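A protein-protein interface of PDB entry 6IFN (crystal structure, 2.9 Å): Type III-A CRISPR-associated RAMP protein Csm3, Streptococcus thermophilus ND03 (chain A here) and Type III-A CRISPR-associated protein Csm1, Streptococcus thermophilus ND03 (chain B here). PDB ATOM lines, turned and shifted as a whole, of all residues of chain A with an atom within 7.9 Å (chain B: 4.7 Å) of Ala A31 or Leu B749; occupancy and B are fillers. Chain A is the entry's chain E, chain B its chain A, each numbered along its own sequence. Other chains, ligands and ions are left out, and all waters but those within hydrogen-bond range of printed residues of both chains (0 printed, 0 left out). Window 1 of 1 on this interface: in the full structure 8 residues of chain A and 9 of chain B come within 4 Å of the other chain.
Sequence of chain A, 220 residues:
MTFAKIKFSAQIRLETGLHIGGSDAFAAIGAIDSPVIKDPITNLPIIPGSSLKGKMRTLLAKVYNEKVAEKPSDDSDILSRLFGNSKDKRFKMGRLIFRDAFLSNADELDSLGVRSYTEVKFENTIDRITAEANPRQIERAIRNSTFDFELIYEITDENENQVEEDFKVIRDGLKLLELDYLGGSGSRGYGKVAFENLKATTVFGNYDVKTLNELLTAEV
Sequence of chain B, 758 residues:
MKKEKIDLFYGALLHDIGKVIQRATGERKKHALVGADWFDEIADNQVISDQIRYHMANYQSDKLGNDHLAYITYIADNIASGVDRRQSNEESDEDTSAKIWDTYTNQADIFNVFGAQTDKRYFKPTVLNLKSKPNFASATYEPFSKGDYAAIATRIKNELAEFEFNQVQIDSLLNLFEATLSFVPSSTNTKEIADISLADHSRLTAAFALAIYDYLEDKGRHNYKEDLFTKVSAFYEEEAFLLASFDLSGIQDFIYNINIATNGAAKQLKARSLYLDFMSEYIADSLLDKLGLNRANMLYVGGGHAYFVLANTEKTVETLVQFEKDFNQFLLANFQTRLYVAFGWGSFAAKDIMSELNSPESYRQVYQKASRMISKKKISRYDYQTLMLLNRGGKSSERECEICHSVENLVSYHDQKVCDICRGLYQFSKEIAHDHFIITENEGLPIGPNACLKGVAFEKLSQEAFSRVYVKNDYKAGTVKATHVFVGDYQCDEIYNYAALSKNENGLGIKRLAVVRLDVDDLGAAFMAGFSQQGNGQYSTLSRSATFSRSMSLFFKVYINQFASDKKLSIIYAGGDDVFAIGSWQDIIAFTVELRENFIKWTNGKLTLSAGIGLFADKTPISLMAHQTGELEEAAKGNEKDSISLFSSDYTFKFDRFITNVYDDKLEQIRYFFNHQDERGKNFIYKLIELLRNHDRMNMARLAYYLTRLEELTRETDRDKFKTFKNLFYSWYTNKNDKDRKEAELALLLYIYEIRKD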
ATOM      1  N   ALA A  27      34.171  24.708 -27.337  1.00  0.00           N
ATOM      2  CA  ALA A  27      34.840  23.494 -27.840  1.00  0.00           C
ATOM      3  C   ALA A  27      35.310  22.576 -26.697  1.00  0.00           C
ATOM      4  O   ALA A  27      35.870  21.522 -26.996  1.00  0.00           O
ATOM      5  CB  ALA A  27      35.996  23.867 -28.760  1.00  0.00           C
ATOM      6  N   ALA A  28      35.104  22.956 -25.423  1.00  0.00           N
ATOM      7  CA  ALA A  28      35.543  22.149 -24.267  1.00  0.00           C
ATOM      8  C   ALA A  28      34.414  21.255 -23.763  1.00  0.00           C
ATOM      9  O   ALA A  28      34.637  20.438 -22.877  1.00  0.00           O
ATOM     10  CB  ALA A  28      36.034  23.014 -23.132  1.00  0.00           C
ATOM     11  N   ILE A  29      33.216  21.418 -24.324  1.00  0.00           N
ATOM     12  CA  ILE A  29      31.988  20.755 -23.807  1.00  0.00           C
ATOM     13  C   ILE A  29      32.143  19.223 -23.869  1.00  0.00           C
ATOM     14  O   ILE A  29      32.541  18.681 -24.897  1.00  0.00           O
ATOM     15  CB  ILE A  29      30.750  21.272 -24.575  1.00  0.00           C
ATOM     16  CG1 ILE A  29      29.597  21.550 -23.609  1.00  0.00           C
ATOM     17  CG2 ILE A  29      30.347  20.358 -25.733  1.00  0.00           C
ATOM     18  CD1 ILE A  29      29.913  22.605 -22.570  1.00  0.00           C
ATOM     19  N   GLY A  30      31.851  18.538 -22.754  1.00  0.00           N
ATOM     20  CA  GLY A  30      32.359  17.161 -22.473  1.00  0.00           C
ATOM     21  C   GLY A  30      31.616  16.038 -23.190  1.00  0.00           C
ATOM     22  O   GLY A  30      31.864  14.854 -22.926  1.00  0.00           O
ATOM     23  N   ALA A  31      30.735  16.398 -24.128  1.00  0.00           N
ATOM     24  CA  ALA A  31      30.033  15.441 -24.983  1.00  0.00           C
ATOM     25  C   ALA A  31      30.970  14.387 -25.597  1.00  0.00           C
ATOM     26  O   ALA A  31      30.488  13.441 -26.188  1.00  0.00           O
ATOM     27  CB  ALA A  31      29.319  16.194 -26.069  1.00  0.00           C
ATOM     28  N   ILE A  32      32.286  14.610 -25.527  1.00  0.00           N
ATOM     29  CA  ILE A  32      33.333  13.628 -25.802  1.00  0.00           C
ATOM     30  C   ILE A  32      34.468  13.933 -24.831  1.00  0.00           C
ATOM     31  O   ILE A  32      34.637  15.083 -24.487  1.00  0.00           O
ATOM     32  CB  ILE A  32      33.847  13.736 -27.251  1.00  0.00           C
ATOM     33  CG1 ILE A  32      34.151  15.199 -27.601  1.00  0.00           C
ATOM     34  CG2 ILE A  32      32.880  13.080 -28.228  1.00  0.00           C
ATOM     35  CD1 ILE A  32      34.442  15.457 -29.053  1.00  0.00           C
ATOM     36  N   ASP A  33      35.289  12.948 -24.482  1.00  0.00           N
ATOM     37  CA  ASP A  33      36.271  13.140 -23.419  1.00  0.00           C
ATOM     38  C   ASP A  33      37.369  14.134 -23.831  1.00  0.00           C
ATOM     39  O   ASP A  33      37.660  15.061 -23.089  1.00  0.00           O
ATOM     40  CB  ASP A  33      36.892  11.807 -23.006  1.00  0.00           C
ATOM     41  CG  ASP A  33      35.886  10.834 -22.415  1.00  0.00           C
ATOM     42  OD1 ASP A  33      35.001  10.365 -23.160  1.00  0.00           O
ATOM     43  OD2 ASP A  33      36.000  10.538 -21.209  1.00  0.00           O
ATOM     44  N   SER A  34      37.986  13.909 -24.994  1.00  0.00           N
ATOM     45  CA  SER A  34      39.185  14.606 -25.378  1.00  0.00           C
ATOM     46  C   SER A  34      38.934  15.340 -26.695  1.00  0.00           C
ATOM     47  O   SER A  34      39.334  14.907 -27.774  1.00  0.00           O
ATOM     48  CB  SER A  34      40.332  13.633 -25.438  1.00  0.00           C
ATOM     49  OG  SER A  34      41.469  14.236 -26.021  1.00  0.00           O
ATOM     50  N   PRO A  35      38.282  16.518 -26.656  1.00  0.00           N
ATOM     51  CA  PRO A  35      37.821  17.181 -27.873  1.00  0.00           C
ATOM     52  C   PRO A  35      39.000  17.820 -28.608  1.00  0.00           C
ATOM     53  O   PRO A  35      40.082  17.829 -28.078  1.00  0.00           O
ATOM     54  CB  PRO A  35      36.886  18.257 -27.335  1.00  0.00           C
ATOM     55  CG  PRO A  35      37.509  18.633 -26.017  1.00  0.00           C
ATOM     56  CD  PRO A  35      38.024  17.324 -25.456  1.00  0.00           C
ATOM     57  N   VAL A 120      35.859   9.521 -33.680  1.00  0.00           N
ATOM     58  CA  VAL A 120      36.143   9.237 -32.297  1.00  0.00           C
ATOM     59  C   VAL A 120      36.969   7.963 -32.213  1.00  0.00           C
ATOM     60  O   VAL A 120      36.440   6.905 -32.485  1.00  0.00           O
ATOM     61  CB  VAL A 120      34.829   9.056 -31.529  1.00  0.00           C
ATOM     62  CG1 VAL A 120      35.059   8.752 -30.061  1.00  0.00           C
ATOM     63  CG2 VAL A 120      33.926  10.266 -31.706  1.00  0.00           C
ATOM     64  N   GLN A 137      38.566   7.148 -25.087  1.00  0.00           N
ATOM     65  CA  GLN A 137      38.136   7.679 -26.387  1.00  0.00           C
ATOM     66  C   GLN A 137      38.725   9.068 -26.572  1.00  0.00           C
ATOM     67  O   GLN A 137      38.758   9.833 -25.621  1.00  0.00           O
ATOM     68  CB  GLN A 137      36.619   7.746 -26.517  1.00  0.00           C
ATOM     69  CG  GLN A 137      35.945   8.387 -25.325  1.00  0.00           C
ATOM     70  CD  GLN A 137      34.503   8.677 -25.656  1.00  0.00           C
ATOM     71  OE1 GLN A 137      34.106   9.825 -25.881  1.00  0.00           O
ATOM     72  NE2 GLN A 137      33.723   7.611 -25.740  1.00  0.00           N
ATOM     73  N   PHE B 647      26.754  26.250 -18.481  1.00  0.00           N
ATOM     74  CA  PHE B 647      27.883  25.852 -19.376  1.00  0.00           C
ATOM     75  C   PHE B 647      27.922  26.234 -20.855  1.00  0.00           C
ATOM     76  O   PHE B 647      28.904  25.924 -21.497  1.00  0.00           O
ATOM     77  CB  PHE B 647      28.044  24.332 -19.499  1.00  0.00           C
ATOM     78  CG  PHE B 647      27.758  23.595 -18.224  1.00  0.00           C
ATOM     79  CD1 PHE B 647      27.933  24.228 -17.011  1.00  0.00           C
ATOM     80  CD2 PHE B 647      27.179  22.349 -18.235  1.00  0.00           C
ATOM     81  CE1 PHE B 647      27.611  23.597 -15.829  1.00  0.00           C
ATOM     82  CE2 PHE B 647      26.855  21.717 -17.052  1.00  0.00           C
ATOM     83  CZ  PHE B 647      27.078  22.340 -15.856  1.00  0.00           C
ATOM     84  N   TYR B 651      22.440  25.976 -23.664  1.00  0.00           N
ATOM     85  CA  TYR B 651      21.685  25.311 -22.595  1.00  0.00           C
ATOM     86  C   TYR B 651      21.081  26.339 -21.637  1.00  0.00           C
ATOM     87  O   TYR B 651      21.647  26.617 -20.595  1.00  0.00           O
ATOM     88  CB  TYR B 651      22.580  24.377 -21.796  1.00  0.00           C
ATOM     89  CG  TYR B 651      23.291  23.345 -22.626  1.00  0.00           C
ATOM     90  CD1 TYR B 651      22.593  22.362 -23.292  1.00  0.00           C
ATOM     91  CD2 TYR B 651      24.667  23.343 -22.711  1.00  0.00           C
ATOM     92  CE1 TYR B 651      23.247  21.399 -24.033  1.00  0.00           C
ATOM     93  CE2 TYR B 651      25.335  22.390 -23.448  1.00  0.00           C
ATOM     94  CZ  TYR B 651      24.624  21.416 -24.114  1.00  0.00           C
ATOM     95  OH  TYR B 651      25.291  20.474 -24.839  1.00  0.00           O
ATOM     96  N   TYR B 686      27.197   8.841 -25.759  1.00  0.00           N
ATOM     97  CA  TYR B 686      27.832   9.667 -26.758  1.00  0.00           C
ATOM     98  C   TYR B 686      26.998   9.661 -28.031  1.00  0.00           C
ATOM     99  O   TYR B 686      26.717  10.721 -28.554  1.00  0.00           O
ATOM    100  CB  TYR B 686      29.273   9.216 -26.964  1.00  0.00           C
ATOM    101  CG  TYR B 686      30.068   9.339 -25.684  1.00  0.00           C
ATOM    102  CD1 TYR B 686      30.071  10.532 -24.980  1.00  0.00           C
ATOM    103  CD2 TYR B 686      30.758   8.267 -25.128  1.00  0.00           C
ATOM    104  CE1 TYR B 686      30.781  10.678 -23.804  1.00  0.00           C
ATOM    105  CE2 TYR B 686      31.469   8.401 -23.943  1.00  0.00           C
ATOM    106  CZ  TYR B 686      31.478   9.613 -23.281  1.00  0.00           C
ATOM    107  OH  TYR B 686      32.167   9.801 -22.124  1.00  0.00           O
ATOM    108  N   ILE B 689      23.932  11.857 -27.490  1.00  0.00           N
ATOM    109  CA  ILE B 689      24.348  13.239 -27.545  1.00  0.00           C
ATOM    110  C   ILE B 689      24.414  13.688 -29.002  1.00  0.00           C
ATOM    111  O   ILE B 689      23.760  14.641 -29.402  1.00  0.00           O
ATOM    112  CB  ILE B 689      25.706  13.407 -26.850  1.00  0.00           C
ATOM    113  CG1 ILE B 689      25.533  13.424 -25.333  1.00  0.00           C
ATOM    114  CG2 ILE B 689      26.447  14.642 -27.340  1.00  0.00           C
ATOM    115  CD1 ILE B 689      24.401  14.291 -24.872  1.00  0.00           C
ATOM    116  N   ARG B 693      22.337  16.604 -31.241  1.00  0.00           N
ATOM    117  CA  ARG B 693      22.893  17.805 -31.842  1.00  0.00           C
ATOM    118  C   ARG B 693      22.563  17.837 -33.338  1.00  0.00           C
ATOM    119  O   ARG B 693      22.488  18.906 -33.927  1.00  0.00           O
ATOM    120  CB  ARG B 693      24.384  17.925 -31.507  1.00  0.00           C
ATOM    121  CG  ARG B 693      24.612  18.403 -30.078  1.00  0.00           C
ATOM    122  CD  ARG B 693      26.059  18.426 -29.624  1.00  0.00           C
ATOM    123  NE  ARG B 693      26.196  18.481 -28.166  1.00  0.00           N
ATOM    124  CZ  ARG B 693      27.349  18.357 -27.500  1.00  0.00           C
ATOM    125  NH1 ARG B 693      28.476  18.119 -28.153  1.00  0.00           N
ATOM    126  NH2 ARG B 693      27.374  18.475 -26.180  1.00  0.00           N
ATOM    127  N   GLU B 745      19.648  16.653 -23.963  1.00  0.00           N
ATOM    128  CA  GLU B 745      21.072  16.851 -24.263  1.00  0.00           C
ATOM    129  C   GLU B 745      21.781  17.233 -22.956  1.00  0.00           C
ATOM    130  O   GLU B 745      22.746  16.608 -22.568  1.00  0.00           O
ATOM    131  CB  GLU B 745      21.259  17.900 -25.375  1.00  0.00           C
ATOM    132  CG  GLU B 745      22.696  18.091 -25.876  1.00  0.00           C
ATOM    133  CD  GLU B 745      22.870  19.147 -26.975  1.00  0.00           C
ATOM    134  OE1 GLU B 745      23.914  19.865 -26.994  1.00  0.00           O
ATOM    135  OE2 GLU B 745      21.970  19.257 -27.835  1.00  0.00           O
ATOM    136  N   LEU B 746      21.237  18.238 -22.262  1.00  0.00           N
ATOM    137  CA  LEU B 746      21.843  18.781 -21.074  1.00  0.00           C
ATOM    138  C   LEU B 746      21.894  17.744 -19.938  1.00  0.00           C
ATOM    139  O   LEU B 746      22.858  17.698 -19.189  1.00  0.00           O
ATOM    140  CB  LEU B 746      21.047  19.999 -20.623  1.00  0.00           C
ATOM    141  CG  LEU B 746      21.551  20.600 -19.321  1.00  0.00           C
ATOM    142  CD1 LEU B 746      23.023  20.982 -19.457  1.00  0.00           C
ATOM    143  CD2 LEU B 746      20.691  21.787 -18.923  1.00  0.00           C
ATOM    144  N   ALA B 747      20.858  16.913 -19.784  1.00  0.00           N
ATOM    145  CA  ALA B 747      20.864  15.893 -18.695  1.00  0.00           C
ATOM    146  C   ALA B 747      21.879  14.798 -19.019  1.00  0.00           C
ATOM    147  O   ALA B 747      22.568  14.362 -18.151  1.00  0.00           O
ATOM    148  CB  ALA B 747      19.497  15.313 -18.451  1.00  0.00           C
ATOM    149  N   LEU B 748      21.986  14.383 -20.278  1.00  0.00           N
ATOM    150  CA  LEU B 748      22.994  13.407 -20.631  1.00  0.00           C
ATOM    151  C   LEU B 748      24.370  13.978 -20.288  1.00  0.00           C
ATOM    152  O   LEU B 748      25.205  13.267 -19.762  1.00  0.00           O
ATOM    153  CB  LEU B 748      22.887  13.067 -22.123  1.00  0.00           C
ATOM    154  CG  LEU B 748      21.825  12.029 -22.527  1.00  0.00           C
ATOM    155  CD1 LEU B 748      21.286  12.272 -23.928  1.00  0.00           C
ATOM    156  CD2 LEU B 748      22.355  10.605 -22.427  1.00  0.00           C
ATOM    157  N   LEU B 749      24.571  15.269 -20.576  1.00  0.00           N
ATOM    158  CA  LEU B 749      25.828  15.989 -20.244  1.00  0.00           C
ATOM    159  C   LEU B 749      26.121  15.954 -18.750  1.00  0.00           C
ATOM    160  O   LEU B 749      27.164  15.516 -18.332  1.00  0.00           O
ATOM    161  CB  LEU B 749      25.738  17.454 -20.651  1.00  0.00           C
ATOM    162  CG  LEU B 749      26.606  17.854 -21.823  1.00  0.00           C
ATOM    163  CD1 LEU B 749      26.823  19.348 -21.786  1.00  0.00           C
ATOM    164  CD2 LEU B 749      27.937  17.115 -21.808  1.00  0.00           C
ATOM    165  N   LEU B 750      25.172  16.459 -17.964  1.00  0.00           N
ATOM    166  CA  LEU B 750      25.289  16.416 -16.532  1.00  0.00           C
ATOM    167  C   LEU B 750      25.731  15.009 -16.115  1.00  0.00           C
ATOM    168  O   LEU B 750      26.684  14.880 -15.379  1.00  0.00           O
ATOM    169  CB  LEU B 750      23.958  16.839 -15.897  1.00  0.00           C
ATOM    170  CG  LEU B 750      23.663  18.343 -15.936  1.00  0.00           C
ATOM    171  CD1 LEU B 750      22.391  18.709 -15.186  1.00  0.00           C
ATOM    172  CD2 LEU B 750      24.823  19.129 -15.346  1.00  0.00           C
ATOM    173  N   TYR B 751      25.077  13.974 -16.647  1.00  0.00           N
ATOM    174  CA  TYR B 751      25.373  12.615 -16.262  1.00  0.00           C
ATOM    175  C   TYR B 751      26.839  12.294 -16.582  1.00  0.00           C
ATOM    176  O   TYR B 751      27.561  11.804 -15.706  1.00  0.00           O
ATOM    177  CB  TYR B 751      24.412  11.606 -16.902  1.00  0.00           C
ATOM    178  CG  TYR B 751      24.700  10.188 -16.477  1.00  0.00           C
ATOM    179  CD1 TYR B 751      24.475   9.767 -15.178  1.00  0.00           C
ATOM    180  CD2 TYR B 751      25.283   9.292 -17.351  1.00  0.00           C
ATOM    181  CE1 TYR B 751      24.812   8.486 -14.770  1.00  0.00           C
ATOM    182  CE2 TYR B 751      25.612   8.006 -16.963  1.00  0.00           C
ATOM    183  CZ  TYR B 751      25.386   7.601 -15.666  1.00  0.00           C
ATOM    184  OH  TYR B 751      25.715   6.330 -15.295  1.00  0.00           O
ATOM    185  N   ILE B 752      27.295  12.598 -17.803  1.00  0.00           N
ATOM    186  CA  ILE B 752      28.652  12.213 -18.212  1.00  0.00           C
ATOM    187  C   ILE B 752      29.691  12.898 -17.314  1.00  0.00           C
ATOM    188  O   ILE B 752      30.569  12.231 -16.798  1.00  0.00           O
ATOM    189  CB  ILE B 752      28.925  12.544 -19.681  1.00  0.00           C
ATOM    190  CG1 ILE B 752      27.991  11.784 -20.622  1.00  0.00           C
ATOM    191  CG2 ILE B 752      30.386  12.270 -19.978  1.00  0.00           C
ATOM    192  CD1 ILE B 752      27.971  12.320 -22.048  1.00  0.00           C
ATOM    193  N   TYR B 753      29.585  14.224 -17.152  1.00  0.00           N
ATOM    194  CA  TYR B 753      30.410  14.972 -16.211  1.00  0.00           C
ATOM    195  C   TYR B 753      30.405  14.287 -14.845  1.00  0.00           C
ATOM    196  O   TYR B 753      31.407  14.264 -14.166  1.00  0.00           O
ATOM    197  CB  TYR B 753      29.896  16.402 -16.005  1.00  0.00           C
ATOM    198  CG  TYR B 753      29.949  17.316 -17.208  1.00  0.00           C
ATOM    199  CD1 TYR B 753      30.810  17.071 -18.260  1.00  0.00           C
ATOM    200  CD2 TYR B 753      29.143  18.444 -17.283  1.00  0.00           C
ATOM    201  CE1 TYR B 753      30.856  17.908 -19.358  1.00  0.00           C
ATOM    202  CE2 TYR B 753      29.182  19.296 -18.375  1.00  0.00           C
ATOM    203  CZ  TYR B 753      30.040  19.022 -19.426  1.00  0.00           C
ATOM    204  OH  TYR B 753      30.109  19.831 -20.533  1.00  0.00           O
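The side-chain hydroxyl of Tyr B651 is in hydrogen-bond range of the guanidinium group of Arg B693, 3.2 Å away.
The side-chain carboxylate of Asp A33 lies close to the side-chain amide oxygen of Gln A137, at 2.9 Å.
The guanidinium group of Arg B693 is in salt-bridge range of the side-chain carboxylate of Glu B745 (2.9 Å).
Among the printed residues, pairs that only touch across the chains: Ile A29 with Phe B647, Ile A29 with Arg B693, Ile A29 with Leu B749, Ile A29 with Tyr B753, Ala A31 with Tyr B686, Ala A31 with Ile B689, Ala A31 with Arg B693, Ala A31 with Leu B749 and Gln A137 with Tyr B686.
Of the printed residues of chain B, Ile A29 touches Phe B647 (3.6 Å), Arg B693 (3.5 Å), Leu B749 (3.98 Å) and Tyr B753 (3.4 Å).
Of the printed residues of chain B, Gly A30 touches Tyr B753.
Of chain B, only Tyr B686 (3.2 Å), Ile B689 (3.5 Å), Arg B693 (3.0 Å) and Leu B749 (3.7 Å) come within 4 Å of Ala A31.
Printed residues of chain B within 4 Å of Gln A137: Tyr B686 (3.0 Å).
Of the printed residues of chain A, Arg B693 touches Ile A29 and Ala A31.
Leu B746 touches none of the printed residues of chain A.
Ala B747 touches none of the printed residues of chain A.
Of the printed residues of chain A, Tyr B753 touches Ile A29 and Gly A30.
The nearest printed residue of chain B that does not touch Ala A31 is Ile B752 (4.8 Å).
The nearest printed residue of chain A that does not touch Leu B749 is Gly A30 (4.1 Å).
The nearest printed residue of chain A that does not touch Ile B689 is Ile A32 (6.1 Å).
OH of Tyr B753 is in hydrogen-bond range of N of Gly A30 (3.1 Å).
OH of Tyr B686 sits at hydrogen-bond distance from OD1 of Asp A33 (3.1 Å).
Printed residues of chain A that touch a printed residue of chain B: Ile A29, Gly A30, Ala A31, Asp A33 and Gln A137.
Among the printed residues, 11 pairs touch across the chains.
Among the printed residues, no Asp or Glu carboxylate lies within 4 Å of a Lys or Arg side-chain nitrogen of the other chain.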
